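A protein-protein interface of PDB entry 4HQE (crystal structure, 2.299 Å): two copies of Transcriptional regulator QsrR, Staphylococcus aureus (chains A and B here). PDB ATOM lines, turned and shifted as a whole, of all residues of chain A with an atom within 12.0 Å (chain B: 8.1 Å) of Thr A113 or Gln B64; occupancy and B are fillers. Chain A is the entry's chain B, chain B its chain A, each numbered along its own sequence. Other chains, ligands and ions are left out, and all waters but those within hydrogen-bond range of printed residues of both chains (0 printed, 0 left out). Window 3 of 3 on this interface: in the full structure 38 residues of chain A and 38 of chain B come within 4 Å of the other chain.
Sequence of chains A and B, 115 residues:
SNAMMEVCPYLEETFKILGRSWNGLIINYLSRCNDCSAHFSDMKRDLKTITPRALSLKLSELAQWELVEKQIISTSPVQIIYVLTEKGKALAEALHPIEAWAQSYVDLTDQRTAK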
ATOM      1  N   TRP A 101     -17.890   4.835  -4.862  1.00  0.00           N
ATOM      2  CA  TRP A 101     -18.118   3.655  -5.699  1.00  0.00           C
ATOM      3  C   TRP A 101     -16.866   2.760  -5.767  1.00  0.00           C
ATOM      4  O   TRP A 101     -16.956   1.543  -5.588  1.00  0.00           O
ATOM      5  CB  TRP A 101     -18.527   4.073  -7.112  1.00  0.00           C
ATOM      6  CG  TRP A 101     -18.756   2.895  -8.009  1.00  0.00           C
ATOM      7  CD1 TRP A 101     -19.914   2.185  -8.149  1.00  0.00           C
ATOM      8  CD2 TRP A 101     -17.792   2.269  -8.878  1.00  0.00           C
ATOM      9  NE1 TRP A 101     -19.734   1.156  -9.047  1.00  0.00           N
ATOM     10  CE2 TRP A 101     -18.446   1.190  -9.515  1.00  0.00           C
ATOM     11  CE3 TRP A 101     -16.444   2.522  -9.175  1.00  0.00           C
ATOM     12  CZ2 TRP A 101     -17.792   0.353 -10.440  1.00  0.00           C
ATOM     13  CZ3 TRP A 101     -15.797   1.693 -10.097  1.00  0.00           C
ATOM     14  CH2 TRP A 101     -16.472   0.617 -10.713  1.00  0.00           C
ATOM     15  N   TYR A 105     -16.792  -1.138  -4.637  1.00  0.00           N
ATOM     16  CA  TYR A 105     -16.976  -2.122  -5.705  1.00  0.00           C
ATOM     17  C   TYR A 105     -15.703  -2.676  -6.374  1.00  0.00           C
ATOM     18  O   TYR A 105     -15.753  -3.721  -7.031  1.00  0.00           O
ATOM     19  CB  TYR A 105     -17.870  -1.521  -6.794  1.00  0.00           C
ATOM     20  CG  TYR A 105     -19.325  -1.429  -6.413  1.00  0.00           C
ATOM     21  CD1 TYR A 105     -20.175  -2.522  -6.568  1.00  0.00           C
ATOM     22  CD2 TYR A 105     -19.855  -0.252  -5.902  1.00  0.00           C
ATOM     23  CE1 TYR A 105     -21.526  -2.437  -6.224  1.00  0.00           C
ATOM     24  CE2 TYR A 105     -21.196  -0.155  -5.554  1.00  0.00           C
ATOM     25  CZ  TYR A 105     -22.029  -1.245  -5.718  1.00  0.00           C
ATOM     26  OH  TYR A 105     -23.364  -1.137  -5.376  1.00  0.00           O
ATOM     27  N   VAL A 106     -14.585  -1.969  -6.230  1.00  0.00           N
ATOM     28  CA  VAL A 106     -13.344  -2.366  -6.875  1.00  0.00           C
ATOM     29  C   VAL A 106     -12.527  -3.312  -5.994  1.00  0.00           C
ATOM     30  O   VAL A 106     -12.319  -3.049  -4.804  1.00  0.00           O
ATOM     31  CB  VAL A 106     -12.471  -1.148  -7.251  1.00  0.00           C
ATOM     32  CG1 VAL A 106     -11.098  -1.598  -7.786  1.00  0.00           C
ATOM     33  CG2 VAL A 106     -13.184  -0.266  -8.271  1.00  0.00           C
ATOM     34  N   ASP A 107     -12.073  -4.411  -6.593  1.00  0.00           N
ATOM     35  CA  ASP A 107     -11.192  -5.347  -5.924  1.00  0.00           C
ATOM     36  C   ASP A 107      -9.845  -5.315  -6.651  1.00  0.00           C
ATOM     37  O   ASP A 107      -9.746  -5.692  -7.822  1.00  0.00           O
ATOM     38  CB  ASP A 107     -11.817  -6.755  -5.929  1.00  0.00           C
ATOM     39  CG  ASP A 107     -10.933  -7.810  -5.238  1.00  0.00           C
ATOM     40  OD1 ASP A 107      -9.725  -7.568  -5.014  1.00  0.00           O
ATOM     41  OD2 ASP A 107     -11.454  -8.908  -4.938  1.00  0.00           O
ATOM     42  N   LEU A 108      -8.812  -4.876  -5.939  1.00  0.00           N
ATOM     43  CA  LEU A 108      -7.495  -4.668  -6.527  1.00  0.00           C
ATOM     44  C   LEU A 108      -6.780  -5.969  -6.885  1.00  0.00           C
ATOM     45  O   LEU A 108      -5.767  -5.952  -7.597  1.00  0.00           O
ATOM     46  CB  LEU A 108      -6.647  -3.799  -5.585  1.00  0.00           C
ATOM     47  CG  LEU A 108      -7.309  -2.438  -5.341  1.00  0.00           C
ATOM     48  CD1 LEU A 108      -6.688  -1.702  -4.168  1.00  0.00           C
ATOM     49  CD2 LEU A 108      -7.242  -1.583  -6.609  1.00  0.00           C
ATOM     50  N   THR A 109      -7.307  -7.095  -6.403  1.00  0.00           N
ATOM     51  CA  THR A 109      -6.728  -8.406  -6.728  1.00  0.00           C
ATOM     52  C   THR A 109      -7.284  -8.974  -8.037  1.00  0.00           C
ATOM     53  O   THR A 109      -6.780  -9.985  -8.541  1.00  0.00           O
ATOM     54  CB  THR A 109      -6.950  -9.443  -5.608  1.00  0.00           C
ATOM     55  OG1 THR A 109      -8.338  -9.783  -5.533  1.00  0.00           O
ATOM     56  CG2 THR A 109      -6.490  -8.895  -4.257  1.00  0.00           C
ATOM     57  N   ASP A 110      -8.321  -8.335  -8.576  1.00  0.00           N
ATOM     58  CA  ASP A 110      -8.946  -8.826  -9.801  1.00  0.00           C
ATOM     59  C   ASP A 110      -7.977  -8.806 -10.985  1.00  0.00           C
ATOM     60  O   ASP A 110      -7.235  -7.829 -11.199  1.00  0.00           O
ATOM     61  CB  ASP A 110     -10.230  -8.054 -10.142  1.00  0.00           C
ATOM     62  CG  ASP A 110     -11.420  -8.430  -9.237  1.00  0.00           C
ATOM     63  OD1 ASP A 110     -12.390  -7.633  -9.150  1.00  0.00           O
ATOM     64  OD2 ASP A 110     -11.393  -9.518  -8.615  1.00  0.00           O
ATOM     65  N   GLN A 111      -7.973  -9.908 -11.731  1.00  0.00           N
ATOM     66  CA  GLN A 111      -7.174 -10.021 -12.943  1.00  0.00           C
ATOM     67  C   GLN A 111      -8.088  -9.879 -14.156  1.00  0.00           C
ATOM     68  O   GLN A 111      -9.232 -10.350 -14.132  1.00  0.00           O
ATOM     69  CB  GLN A 111      -6.467 -11.386 -12.976  1.00  0.00           C
ATOM     70  CG  GLN A 111      -5.685 -11.688 -11.699  1.00  0.00           C
ATOM     71  CD  GLN A 111      -4.557 -10.710 -11.498  1.00  0.00           C
ATOM     72  OE1 GLN A 111      -3.640 -10.626 -12.327  1.00  0.00           O
ATOM     73  NE2 GLN A 111      -4.614  -9.947 -10.401  1.00  0.00           N
ATOM     74  N   ARG A 112      -7.587  -9.217 -15.197  1.00  0.00           N
ATOM     75  CA  ARG A 112      -8.252  -9.153 -16.499  1.00  0.00           C
ATOM     76  C   ARG A 112      -7.194  -9.374 -17.570  1.00  0.00           C
ATOM     77  O   ARG A 112      -5.995  -9.209 -17.304  1.00  0.00           O
ATOM     78  CB  ARG A 112      -8.841  -7.758 -16.765  1.00  0.00           C
ATOM     79  CG  ARG A 112      -9.865  -7.262 -15.779  1.00  0.00           C
ATOM     80  CD  ARG A 112      -9.926  -5.745 -15.861  1.00  0.00           C
ATOM     81  NE  ARG A 112      -9.536  -5.138 -14.596  1.00  0.00           N
ATOM     82  CZ  ARG A 112      -8.413  -4.451 -14.402  1.00  0.00           C
ATOM     83  NH1 ARG A 112      -7.545  -4.259 -15.395  1.00  0.00           N
ATOM     84  NH2 ARG A 112      -8.163  -3.949 -13.205  1.00  0.00           N
ATOM     85  N   THR A 113      -7.645  -9.710 -18.781  1.00  0.00           N
ATOM     86  CA  THR A 113      -6.803  -9.639 -19.974  1.00  0.00           C
ATOM     87  C   THR A 113      -6.486  -8.186 -20.331  1.00  0.00           C
ATOM     88  O   THR A 113      -7.390  -7.420 -20.682  1.00  0.00           O
ATOM     89  CB  THR A 113      -7.501 -10.258 -21.196  1.00  0.00           C
ATOM     90  OG1 THR A 113      -8.350 -11.336 -20.775  1.00  0.00           O
ATOM     91  CG2 THR A 113      -6.458 -10.754 -22.204  1.00  0.00           C
ATOM     92  N   ILE B  17     -10.752   2.631 -16.218  1.00  0.00           N
ATOM     93  CA  ILE B  17     -11.920   2.520 -17.122  1.00  0.00           C
ATOM     94  C   ILE B  17     -12.454   3.876 -17.550  1.00  0.00           C
ATOM     95  O   ILE B  17     -12.652   4.134 -18.738  1.00  0.00           O
ATOM     96  CB  ILE B  17     -13.123   1.779 -16.497  1.00  0.00           C
ATOM     97  CG1 ILE B  17     -12.781   1.286 -15.103  1.00  0.00           C
ATOM     98  CG2 ILE B  17     -13.575   0.625 -17.418  1.00  0.00           C
ATOM     99  CD1 ILE B  17     -13.928   1.352 -14.148  1.00  0.00           C
ATOM    100  N   SER B  56     -17.038  -2.409 -30.184  1.00  0.00           N
ATOM    101  CA  SER B  56     -16.781  -3.804 -29.825  1.00  0.00           C
ATOM    102  C   SER B  56     -15.659  -3.966 -28.800  1.00  0.00           C
ATOM    103  O   SER B  56     -15.782  -4.736 -27.830  1.00  0.00           O
ATOM    104  CB  SER B  56     -16.452  -4.618 -31.087  1.00  0.00           C
ATOM    105  OG  SER B  56     -16.107  -5.950 -30.755  1.00  0.00           O
ATOM    106  N   LEU B  57     -14.567  -3.246 -29.020  1.00  0.00           N
ATOM    107  CA  LEU B  57     -13.430  -3.254 -28.096  1.00  0.00           C
ATOM    108  C   LEU B  57     -13.858  -2.778 -26.714  1.00  0.00           C
ATOM    109  O   LEU B  57     -13.596  -3.427 -25.699  1.00  0.00           O
ATOM    110  CB  LEU B  57     -12.329  -2.319 -28.613  1.00  0.00           C
ATOM    111  CG  LEU B  57     -11.095  -2.883 -29.323  1.00  0.00           C
ATOM    112  CD1 LEU B  57     -11.180  -4.400 -29.557  1.00  0.00           C
ATOM    113  CD2 LEU B  57     -10.839  -2.134 -30.633  1.00  0.00           C
ATOM    114  N   LYS B  58     -14.525  -1.632 -26.687  1.00  0.00           N
ATOM    115  CA  LYS B  58     -14.996  -1.066 -25.431  1.00  0.00           C
ATOM    116  C   LYS B  58     -15.992  -1.988 -24.726  1.00  0.00           C
ATOM    117  O   LYS B  58     -15.937  -2.144 -23.492  1.00  0.00           O
ATOM    118  CB  LYS B  58     -15.572   0.336 -25.662  1.00  0.00           C
ATOM    119  CG  LYS B  58     -14.520   1.348 -26.088  1.00  0.00           C
ATOM    120  CD  LYS B  58     -13.515   1.601 -24.966  1.00  0.00           C
ATOM    121  CE  LYS B  58     -12.300   2.359 -25.474  1.00  0.00           C
ATOM    122  NZ  LYS B  58     -11.427   2.806 -24.353  1.00  0.00           N
ATOM    123  N   LEU B  59     -16.880  -2.632 -25.486  1.00  0.00           N
ATOM    124  CA  LEU B  59     -17.825  -3.563 -24.848  1.00  0.00           C
ATOM    125  C   LEU B  59     -17.097  -4.784 -24.236  1.00  0.00           C
ATOM    126  O   LEU B  59     -17.496  -5.279 -23.177  1.00  0.00           O
ATOM    127  CB  LEU B  59     -18.961  -3.972 -25.804  1.00  0.00           C
ATOM    128  CG  LEU B  59     -20.050  -2.937 -26.144  1.00  0.00           C
ATOM    129  CD1 LEU B  59     -20.932  -3.413 -27.307  1.00  0.00           C
ATOM    130  CD2 LEU B  59     -20.925  -2.603 -24.933  1.00  0.00           C
ATOM    131  N   SER B  60     -15.996  -5.224 -24.860  1.00  0.00           N
ATOM    132  CA  SER B  60     -15.175  -6.319 -24.287  1.00  0.00           C
ATOM    133  C   SER B  60     -14.439  -5.844 -23.041  1.00  0.00           C
ATOM    134  O   SER B  60     -14.398  -6.558 -22.032  1.00  0.00           O
ATOM    135  CB  SER B  60     -14.151  -6.862 -25.299  1.00  0.00           C
ATOM    136  OG  SER B  60     -14.777  -7.290 -26.493  1.00  0.00           O
ATOM    137  N   GLU B  61     -13.842  -4.650 -23.136  1.00  0.00           N
ATOM    138  CA  GLU B  61     -13.232  -3.966 -21.998  1.00  0.00           C
ATOM    139  C   GLU B  61     -14.220  -3.917 -20.809  1.00  0.00           C
ATOM    140  O   GLU B  61     -13.883  -4.322 -19.695  1.00  0.00           O
ATOM    141  CB  GLU B  61     -12.803  -2.546 -22.436  1.00  0.00           C
ATOM    142  CG  GLU B  61     -11.520  -1.961 -21.798  1.00  0.00           C
ATOM    143  CD  GLU B  61     -11.083  -0.597 -22.427  1.00  0.00           C
ATOM    144  OE1 GLU B  61     -11.247   0.475 -21.789  1.00  0.00           O
ATOM    145  OE2 GLU B  61     -10.557  -0.598 -23.569  1.00  0.00           O
ATOM    146  N   LEU B  62     -15.450  -3.454 -21.054  1.00  0.00           N
ATOM    147  CA  LEU B  62     -16.448  -3.289 -19.981  1.00  0.00           C
ATOM    148  C   LEU B  62     -16.935  -4.609 -19.419  1.00  0.00           C
ATOM    149  O   LEU B  62     -17.313  -4.701 -18.250  1.00  0.00           O
ATOM    150  CB  LEU B  62     -17.640  -2.468 -20.475  1.00  0.00           C
ATOM    151  CG  LEU B  62     -17.303  -0.997 -20.727  1.00  0.00           C
ATOM    152  CD1 LEU B  62     -18.302  -0.393 -21.678  1.00  0.00           C
ATOM    153  CD2 LEU B  62     -17.263  -0.213 -19.405  1.00  0.00           C
ATOM    154  N   ALA B  63     -16.946  -5.633 -20.267  1.00  0.00           N
ATOM    155  CA  ALA B  63     -17.283  -6.969 -19.815  1.00  0.00           C
ATOM    156  C   ALA B  63     -16.212  -7.492 -18.858  1.00  0.00           C
ATOM    157  O   ALA B  63     -16.539  -8.100 -17.825  1.00  0.00           O
ATOM    158  CB  ALA B  63     -17.471  -7.919 -21.007  1.00  0.00           C
ATOM    159  N   GLN B  64     -14.941  -7.263 -19.190  1.00  0.00           N
ATOM    160  CA  GLN B  64     -13.851  -7.698 -18.306  1.00  0.00           C
ATOM    161  C   GLN B  64     -13.981  -7.062 -16.933  1.00  0.00           C
ATOM    162  O   GLN B  64     -13.730  -7.721 -15.916  1.00  0.00           O
ATOM    163  CB  GLN B  64     -12.479  -7.352 -18.900  1.00  0.00           C
ATOM    164  CG  GLN B  64     -12.056  -8.226 -20.085  1.00  0.00           C
ATOM    165  CD  GLN B  64     -11.103  -7.500 -21.027  1.00  0.00           C
ATOM    166  OE1 GLN B  64     -10.146  -6.845 -20.586  1.00  0.00           O
ATOM    167  NE2 GLN B  64     -11.367  -7.605 -22.339  1.00  0.00           N
ATOM    168  N   TRP B  65     -14.376  -5.785 -16.903  1.00  0.00           N
ATOM    169  CA  TRP B  65     -14.582  -5.078 -15.626  1.00  0.00           C
ATOM    170  C   TRP B  65     -15.887  -5.500 -14.966  1.00  0.00           C
ATOM    171  O   TRP B  65     -16.224  -4.998 -13.882  1.00  0.00           O
ATOM    172  CB  TRP B  65     -14.580  -3.557 -15.822  1.00  0.00           C
ATOM    173  CG  TRP B  65     -13.223  -2.993 -16.100  1.00  0.00           C
ATOM    174  CD1 TRP B  65     -12.615  -2.867 -17.327  1.00  0.00           C
ATOM    175  CD2 TRP B  65     -12.299  -2.474 -15.140  1.00  0.00           C
ATOM    176  NE1 TRP B  65     -11.368  -2.297 -17.180  1.00  0.00           N
ATOM    177  CE2 TRP B  65     -11.146  -2.049 -15.845  1.00  0.00           C
ATOM    178  CE3 TRP B  65     -12.331  -2.316 -13.751  1.00  0.00           C
ATOM    179  CZ2 TRP B  65     -10.038  -1.489 -15.207  1.00  0.00           C
ATOM    180  CZ3 TRP B  65     -11.229  -1.753 -13.117  1.00  0.00           C
ATOM    181  CH2 TRP B  65     -10.100  -1.350 -13.844  1.00  0.00           C
ATOM    182  N   GLU B  66     -16.614  -6.407 -15.631  1.00  0.00           N
ATOM    183  CA  GLU B  66     -17.938  -6.848 -15.188  1.00  0.00           C
ATOM    184  C   GLU B  66     -18.900  -5.676 -14.985  1.00  0.00           C
ATOM    185  O   GLU B  66     -19.719  -5.697 -14.058  1.00  0.00           O
ATOM    186  CB  GLU B  66     -17.847  -7.722 -13.924  1.00  0.00           C
ATOM    187  CG  GLU B  66     -17.163  -9.068 -14.181  1.00  0.00           C
ATOM    188  CD  GLU B  66     -16.631  -9.715 -12.911  1.00  0.00           C
ATOM    189  OE1 GLU B  66     -16.311  -8.978 -11.945  1.00  0.00           O
ATOM    190  OE2 GLU B  66     -16.531 -10.964 -12.883  1.00  0.00           O
ATOM    191  N   LEU B  67     -18.809  -4.682 -15.875  1.00  0.00           N
ATOM    192  CA  LEU B  67     -19.698  -3.522 -15.842  1.00  0.00           C
ATOM    193  C   LEU B  67     -20.908  -3.717 -16.770  1.00  0.00           C
ATOM    194  O   LEU B  67     -22.040  -3.325 -16.434  1.00  0.00           O
ATOM    195  CB  LEU B  67     -18.921  -2.254 -16.213  1.00  0.00           C
ATOM    196  CG  LEU B  67     -17.889  -1.800 -15.168  1.00  0.00           C
ATOM    197  CD1 LEU B  67     -17.015  -0.646 -15.668  1.00  0.00           C
ATOM    198  CD2 LEU B  67     -18.582  -1.418 -13.852  1.00  0.00           C
ATOM    199  N   VAL B  68     -20.652  -4.330 -17.930  1.00  0.00           N
ATOM    200  CA  VAL B  68     -21.679  -4.642 -18.924  1.00  0.00           C
ATOM    201  C   VAL B  68     -21.563  -6.109 -19.329  1.00  0.00           C
ATOM    202  O   VAL B  68     -20.520  -6.535 -19.834  1.00  0.00           O
ATOM    203  CB  VAL B  68     -21.488  -3.818 -20.214  1.00  0.00           C
ATOM    204  CG1 VAL B  68     -22.485  -4.254 -21.279  1.00  0.00           C
ATOM    205  CG2 VAL B  68     -21.586  -2.322 -19.926  1.00  0.00           C
ATOM    206  N   GLU B  69     -22.630  -6.875 -19.118  1.00  0.00           N
ATOM    207  CA  GLU B  69     -22.664  -8.281 -19.512  1.00  0.00           C
ATOM    208  C   GLU B  69     -23.189  -8.454 -20.928  1.00  0.00           C
ATOM    209  O   GLU B  69     -24.257  -7.925 -21.268  1.00  0.00           O
ATOM    210  CB  GLU B  69     -23.592  -9.053 -18.594  1.00  0.00           C
ATOM    211  CG  GLU B  69     -22.904  -9.842 -17.505  1.00  0.00           C
ATOM    212  CD  GLU B  69     -23.889 -10.279 -16.437  1.00  0.00           C
ATOM    213  OE1 GLU B  69     -23.590 -10.069 -15.235  1.00  0.00           O
ATOM    214  OE2 GLU B  69     -24.969 -10.807 -16.810  1.00  0.00           O
ATOM    215  N   LYS B  87     -23.263  -3.488 -10.535  1.00  0.00           N
ATOM    216  CA  LYS B  87     -22.023  -2.735 -10.376  1.00  0.00           C
ATOM    217  C   LYS B  87     -21.945  -1.594 -11.395  1.00  0.00           C
ATOM    218  O   LYS B  87     -21.603  -0.441 -11.053  1.00  0.00           O
ATOM    219  CB  LYS B  87     -20.832  -3.676 -10.554  1.00  0.00           C
ATOM    220  CG  LYS B  87     -19.497  -3.064 -10.213  1.00  0.00           C
ATOM    221  CD  LYS B  87     -18.411  -4.139 -10.152  1.00  0.00           C
ATOM    222  CE  LYS B  87     -17.356  -3.902 -11.214  1.00  0.00           C
ATOM    223  NZ  LYS B  87     -16.037  -4.537 -10.861  1.00  0.00           N
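No position is printed for both chains.
Of the 6 pairs that touch across the chains among the printed residues, none has its exchanged pair printed and touching as well.
Among the printed residues, pairs that only touch across the chains: Arg A112 with Trp B65 (3.3 Å), Tyr A105 with Lys B87 (3.7 Å), Arg A112 with Gln B64 (3.9 Å) and Trp A101 with Leu B67 (3.9 Å).
O of Thr A113 sits close to OE1 of Gln B64.
The backbone carbonyl oxygen (O) of Lys B87 lies within hydrogen-bond range of the indole nitrogen (NE1) of Trp A101 (3.2 Å).
The side-chain amide nitrogen of Gln B64 lies within hydrogen-bond range of the backbone carbonyl oxygen of Ser B60, at 3.2 Å.
The backbone carbonyl oxygen (O) of Leu B62 is in hydrogen-bond range of the backbone NH (N) of Leu B67 (2.8 Å).
The backbone carbonyl oxygen (O) of Trp B65 sits at hydrogen-bond distance from the side-chain amino group (NZ) of Lys B87, 3.1 Å away.
Of chain A, only Arg A112 and Thr A113 come within 4 Å of Gln B64.
Ser B60 touches none of the printed residues of chain A.
No residue of chain A comes within 4 Å of Glu B61.
No residue of chain A comes within 4 Å of Ala B63.
Of chain A, only Arg A112 comes within 4 Å of Trp B65.
No residue of chain A comes within 4 Å of Glu B66.
Printed residues of chain A within 4 Å of Leu B67: Trp A101.
Of the printed residues of chain B, Arg A112 touches Gln B64 and Trp B65.
Of the printed residues of chain A, Lys B87 touches Trp A101 and Tyr A105.
The nearest residue of chain A that does not touch Gln B64 is Gln A111 (5.5 Å).
Of the 10 printed residues of chain A, 4 touch a printed residue of chain B.
Along chain A the printed residues that touch a printed residue of chain B span positions 101 to 113.
Hydrophobic or aromatic side chains of chain B within 4 Å of the printed part of chain A: Trp B65 and Leu B67.
Among the printed residues, 6 pairs touch across the chains.
Among the printed residues, no Asp or Glu carboxylate lies within 4 Å of a Lys or Arg side-chain nitrogen of the other chain.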
